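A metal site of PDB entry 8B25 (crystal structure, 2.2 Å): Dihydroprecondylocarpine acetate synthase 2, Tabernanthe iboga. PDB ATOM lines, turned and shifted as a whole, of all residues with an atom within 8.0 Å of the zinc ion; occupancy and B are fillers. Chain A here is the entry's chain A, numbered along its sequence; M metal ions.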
ATOM      1  N   GLY A 103     -15.937 -35.732  17.788  1.00  0.00           N
ATOM      2  CA  GLY A 103     -17.284 -35.188  17.932  1.00  0.00           C
ATOM      3  C   GLY A 103     -17.294 -33.682  17.749  1.00  0.00           C
ATOM      4  O   GLY A 103     -16.244 -33.008  17.719  1.00  0.00           O
ATOM      5  N   THR A 104     -18.525 -33.153  17.648  1.00  0.00           N
ATOM      6  CA  THR A 104     -18.820 -31.736  17.413  1.00  0.00           C
ATOM      7  C   THR A 104     -20.116 -31.402  18.142  1.00  0.00           C
ATOM      8  O   THR A 104     -20.762 -32.284  18.729  1.00  0.00           O
ATOM      9  CB  THR A 104     -18.975 -31.437  15.905  1.00  0.00           C
ATOM     10  OG1 THR A 104     -20.099 -32.169  15.373  1.00  0.00           O
ATOM     11  CG2 THR A 104     -17.702 -31.798  15.148  1.00  0.00           C
ATOM     12  N   CYS A 105     -20.477 -30.113  18.147  1.00  0.00           N
ATOM     13  CA  CYS A 105     -21.674 -29.687  18.899  1.00  0.00           C
ATOM     14  C   CYS A 105     -22.968 -30.180  18.244  1.00  0.00           C
ATOM     15  O   CYS A 105     -24.005 -30.273  18.901  1.00  0.00           O
ATOM     16  CB  CYS A 105     -21.709 -28.162  19.084  1.00  0.00           C
ATOM     17  SG  CYS A 105     -22.330 -27.231  17.625  1.00  0.00           S
ATOM     18  N   GLY A 106     -22.963 -30.442  16.953  1.00  0.00           N
ATOM     19  CA  GLY A 106     -24.156 -30.910  16.305  1.00  0.00           C
ATOM     20  C   GLY A 106     -25.158 -29.823  15.966  1.00  0.00           C
ATOM     21  O   GLY A 106     -26.140 -30.130  15.272  1.00  0.00           O
ATOM     22  N   LYS A 107     -24.934 -28.566  16.378  1.00  0.00           N
ATOM     23  CA  LYS A 107     -25.940 -27.502  16.222  1.00  0.00           C
ATOM     24  C   LYS A 107     -25.469 -26.250  15.445  1.00  0.00           C
ATOM     25  O   LYS A 107     -26.303 -25.598  14.812  1.00  0.00           O
ATOM     26  CB  LYS A 107     -26.460 -27.075  17.612  1.00  0.00           C
ATOM     27  N   CYS A 108     -24.175 -25.957  15.392  1.00  0.00           N
ATOM     28  CA  CYS A 108     -23.710 -24.744  14.716  1.00  0.00           C
ATOM     29  C   CYS A 108     -23.848 -24.879  13.197  1.00  0.00           C
ATOM     30  O   CYS A 108     -24.229 -25.932  12.671  1.00  0.00           O
ATOM     31  CB  CYS A 108     -22.268 -24.419  15.112  1.00  0.00           C
ATOM     32  SG  CYS A 108     -21.072 -25.570  14.228  1.00  0.00           S
ATOM     33  N   TYR A 109     -23.536 -23.791  12.488  1.00  0.00           N
ATOM     34  CA  TYR A 109     -23.600 -23.771  11.018  1.00  0.00           C
ATOM     35  C   TYR A 109     -22.635 -24.794  10.414  1.00  0.00           C
ATOM     36  O   TYR A 109     -22.945 -25.442   9.396  1.00  0.00           O
ATOM     37  CB  TYR A 109     -23.288 -22.358  10.499  1.00  0.00           C
ATOM     38  CG  TYR A 109     -23.368 -22.244   8.997  1.00  0.00           C
ATOM     39  CD1 TYR A 109     -22.328 -22.672   8.217  1.00  0.00           C
ATOM     40  CD2 TYR A 109     -24.515 -21.745   8.355  1.00  0.00           C
ATOM     41  CE1 TYR A 109     -22.391 -22.661   6.850  1.00  0.00           C
ATOM     42  CE2 TYR A 109     -24.565 -21.688   6.964  1.00  0.00           C
ATOM     43  CZ  TYR A 109     -23.478 -22.152   6.217  1.00  0.00           C
ATOM     44  OH  TYR A 109     -23.427 -22.149   4.837  1.00  0.00           O
ATOM     45  N   ASN A 110     -21.404 -24.874  10.939  1.00  0.00           N
ATOM     46  CA  ASN A 110     -20.460 -25.844  10.387  1.00  0.00           C
ATOM     47  C   ASN A 110     -20.987 -27.268  10.536  1.00  0.00           C
ATOM     48  O   ASN A 110     -20.916 -28.058   9.594  1.00  0.00           O
ATOM     49  CB  ASN A 110     -19.103 -25.686  11.050  1.00  0.00           C
ATOM     50  CG  ASN A 110     -18.568 -24.303  10.915  1.00  0.00           C
ATOM     51  OD1 ASN A 110     -18.436 -23.792   9.805  1.00  0.00           O
ATOM     52  ND2 ASN A 110     -18.353 -23.624  12.066  1.00  0.00           N
ATOM     53  N   CYS A 111     -21.523 -27.625  11.707  1.00  0.00           N
ATOM     54  CA  CYS A 111     -21.980 -29.004  11.891  1.00  0.00           C
ATOM     55  C   CYS A 111     -23.168 -29.326  10.990  1.00  0.00           C
ATOM     56  O   CYS A 111     -23.258 -30.437  10.425  1.00  0.00           O
ATOM     57  CB  CYS A 111     -22.354 -29.245  13.348  1.00  0.00           C
ATOM     58  SG  CYS A 111     -20.991 -29.195  14.504  1.00  0.00           S
ATOM     59  N   VAL A 112     -24.103 -28.388  10.846  1.00  0.00           N
ATOM     60  CA  VAL A 112     -25.356 -28.638  10.141  1.00  0.00           C
ATOM     61  C   VAL A 112     -25.144 -28.653   8.643  1.00  0.00           C
ATOM     62  O   VAL A 112     -25.948 -29.236   7.913  1.00  0.00           O
ATOM     63  CB  VAL A 112     -26.363 -27.566  10.633  1.00  0.00           C
ATOM     64  CG1 VAL A 112     -27.343 -27.215   9.608  1.00  0.00           C
ATOM     65  CG2 VAL A 112     -27.035 -28.023  11.936  1.00  0.00           C
ATOM     66  N   LEU A 115     -19.551 -29.410   7.412  1.00  0.00           N
ATOM     67  CA  LEU A 115     -18.227 -28.805   7.478  1.00  0.00           C
ATOM     68  C   LEU A 115     -17.725 -28.879   8.916  1.00  0.00           C
ATOM     69  O   LEU A 115     -17.164 -27.939   9.471  1.00  0.00           O
ATOM     70  CB  LEU A 115     -18.246 -27.354   7.012  1.00  0.00           C
ATOM     71  CG  LEU A 115     -18.810 -27.108   5.615  1.00  0.00           C
ATOM     72  CD1 LEU A 115     -18.942 -25.608   5.269  1.00  0.00           C
ATOM     73  CD2 LEU A 115     -17.884 -27.852   4.630  1.00  0.00           C
ATOM     74  N   GLU A 116     -17.985 -30.002   9.552  1.00  0.00           N
ATOM     75  CA  GLU A 116     -17.966 -30.041  10.999  1.00  0.00           C
ATOM     76  C   GLU A 116     -16.572 -30.041  11.585  1.00  0.00           C
ATOM     77  O   GLU A 116     -16.435 -29.795  12.779  1.00  0.00           O
ATOM     78  CB  GLU A 116     -18.822 -31.244  11.479  1.00  0.00           C
ATOM     79  CG  GLU A 116     -18.178 -32.656  11.284  1.00  0.00           C
ATOM     80  CD  GLU A 116     -17.942 -33.042   9.842  1.00  0.00           C
ATOM     81  OE1 GLU A 116     -18.805 -32.678   8.984  1.00  0.00           O
ATOM     82  OE2 GLU A 116     -16.872 -33.691   9.557  1.00  0.00           O
ATOM     83  N   ASN A 117     -15.523 -30.309  10.777  1.00  0.00           N
ATOM     84  CA  ASN A 117     -14.163 -30.144  11.290  1.00  0.00           C
ATOM     85  C   ASN A 117     -13.875 -28.715  11.759  1.00  0.00           C
ATOM     86  O   ASN A 117     -13.006 -28.523  12.622  1.00  0.00           O
ATOM     87  CB  ASN A 117     -13.115 -30.614  10.252  1.00  0.00           C
ATOM     88  CG  ASN A 117     -13.184 -29.836   8.943  1.00  0.00           C
ATOM     89  OD1 ASN A 117     -14.266 -29.669   8.363  1.00  0.00           O
ATOM     90  ND2 ASN A 117     -12.042 -29.374   8.474  1.00  0.00           N
ATOM     91  N   TYR A 118     -14.656 -27.716  11.315  1.00  0.00           N
ATOM     92  CA  TYR A 118     -14.485 -26.325  11.752  1.00  0.00           C
ATOM     93  C   TYR A 118     -15.501 -25.922  12.815  1.00  0.00           C
ATOM     94  O   TYR A 118     -15.693 -24.721  13.057  1.00  0.00           O
ATOM     95  CB  TYR A 118     -14.568 -25.353  10.560  1.00  0.00           C
ATOM     96  CG  TYR A 118     -13.384 -25.472   9.682  1.00  0.00           C
ATOM     97  CD1 TYR A 118     -12.122 -25.231  10.193  1.00  0.00           C
ATOM     98  CD2 TYR A 118     -13.498 -25.924   8.352  1.00  0.00           C
ATOM     99  CE1 TYR A 118     -10.995 -25.415   9.431  1.00  0.00           C
ATOM    100  CE2 TYR A 118     -12.363 -26.106   7.567  1.00  0.00           C
ATOM    101  CZ  TYR A 118     -11.101 -25.842   8.116  1.00  0.00           C
ATOM    102  OH  TYR A 118      -9.935 -25.974   7.404  1.00  0.00           O
ATOM    103  N   CYS A 119     -16.153 -26.876  13.439  1.00  0.00           N
ATOM    104  CA  CYS A 119     -16.946 -26.541  14.607  1.00  0.00           C
ATOM    105  C   CYS A 119     -16.078 -25.864  15.671  1.00  0.00           C
ATOM    106  O   CYS A 119     -14.959 -26.313  15.941  1.00  0.00           O
ATOM    107  CB  CYS A 119     -17.596 -27.796  15.163  1.00  0.00           C
ATOM    108  SG  CYS A 119     -18.603 -27.682  16.669  1.00  0.00           S
ATOM    109  N   PRO A 120     -16.566 -24.786  16.283  1.00  0.00           N
ATOM    110  CA  PRO A 120     -15.802 -24.160  17.392  1.00  0.00           C
ATOM    111  C   PRO A 120     -15.655 -25.089  18.581  1.00  0.00           C
ATOM    112  O   PRO A 120     -14.771 -24.864  19.422  1.00  0.00           O
ATOM    113  CB  PRO A 120     -16.612 -22.885  17.755  1.00  0.00           C
ATOM    114  CG  PRO A 120     -17.537 -22.663  16.614  1.00  0.00           C
ATOM    115  CD  PRO A 120     -17.797 -24.040  15.962  1.00  0.00           C
ATOM    116  N   GLU A 121     -16.466 -26.144  18.695  1.00  0.00           N
ATOM    117  CA  GLU A 121     -16.342 -27.106  19.786  1.00  0.00           C
ATOM    118  C   GLU A 121     -16.009 -28.521  19.317  1.00  0.00           C
ATOM    119  O   GLU A 121     -16.394 -29.500  19.963  1.00  0.00           O
ATOM    120  CB  GLU A 121     -17.638 -27.123  20.603  1.00  0.00           C
ATOM    121  CG  GLU A 121     -17.868 -25.822  21.410  1.00  0.00           C
ATOM    122  CD  GLU A 121     -19.271 -25.754  21.972  1.00  0.00           C
ATOM    123  OE1 GLU A 121     -19.871 -24.658  21.858  1.00  0.00           O
ATOM    124  OE2 GLU A 121     -19.777 -26.774  22.533  1.00  0.00           O
ATOM    125  N   VAL A 122     -15.229 -28.646  18.232  1.00  0.00           N
ATOM    126  CA  VAL A 122     -14.765 -29.949  17.765  1.00  0.00           C
ATOM    127  C   VAL A 122     -13.963 -30.634  18.869  1.00  0.00           C
ATOM    128  O   VAL A 122     -13.136 -30.016  19.555  1.00  0.00           O
ATOM    129  CB  VAL A 122     -13.935 -29.794  16.481  1.00  0.00           C
ATOM    130  CG1 VAL A 122     -12.653 -28.889  16.729  1.00  0.00           C
ATOM    131  CG2 VAL A 122     -13.542 -31.183  15.875  1.00  0.00           C
ATOM    132  N   ARG A 149     -20.725 -40.981  12.937  1.00  0.00           N
ATOM    133  CA  ARG A 149     -20.483 -39.882  11.993  1.00  0.00           C
ATOM    134  C   ARG A 149     -18.996 -39.722  11.671  1.00  0.00           C
ATOM    135  O   ARG A 149     -18.659 -39.207  10.596  1.00  0.00           O
ATOM    136  CB  ARG A 149     -21.047 -38.547  12.525  1.00  0.00           C
ATOM    137  CG  ARG A 149     -20.989 -37.438  11.463  1.00  0.00           C
ATOM    138  CD  ARG A 149     -21.536 -36.119  12.026  1.00  0.00           C
ATOM    139  NE  ARG A 149     -21.386 -35.006  11.087  1.00  0.00           N
ATOM    140  CZ  ARG A 149     -21.896 -33.805  11.291  1.00  0.00           C
ATOM    141  NH1 ARG A 149     -22.577 -33.508  12.397  1.00  0.00           N
ATOM    142  NH2 ARG A 149     -21.723 -32.862  10.364  1.00  0.00           N
HETATM  143 ZN    ZN M   1     -20.744 -27.263  15.801  1.00  0.00          ZN
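The side-chain sulfur (SG) of Cys 111 sits close to the side-chain hydroxyl (OG1) of Thr 104 (3.2 Å). SG of Cys 111 sits close to N of Gly 106, at 3.4 Å. The backbone NH of Asn 110 sits close to the side-chain sulfur of Cys 108 (3.4 Å). The side-chain sulfur (SG) of Cys 105 sits close to the backbone NH (N) of Lys 107, at 3.2 Å. The backbone NH of Glu 121 lies close to the side-chain sulfur of Cys 119. The guanidinium group of Arg 149 sits at hydrogen-bond distance from the backbone carbonyl oxygen of Cys 111 (2.9 Å).
Four residues have an atom within 4 Å of the zinc ion: Cys 105, Cys 108, Cys 111 and Cys 119. Along chain A the residues within 4 Å of the zinc ion span positions 105 to 119. The nearest printed residue that does not touch the zinc ion is Gly 106 (4.04 Å).
The zinc ion is bound by the side-chain sulfur of Cys 108 (2.3 Å), the side-chain sulfur of Cys 111 (2.3 Å), the side-chain sulfur of Cys 119 (2.3 Å) and the side-chain sulfur of Cys 105 (2.4 Å).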
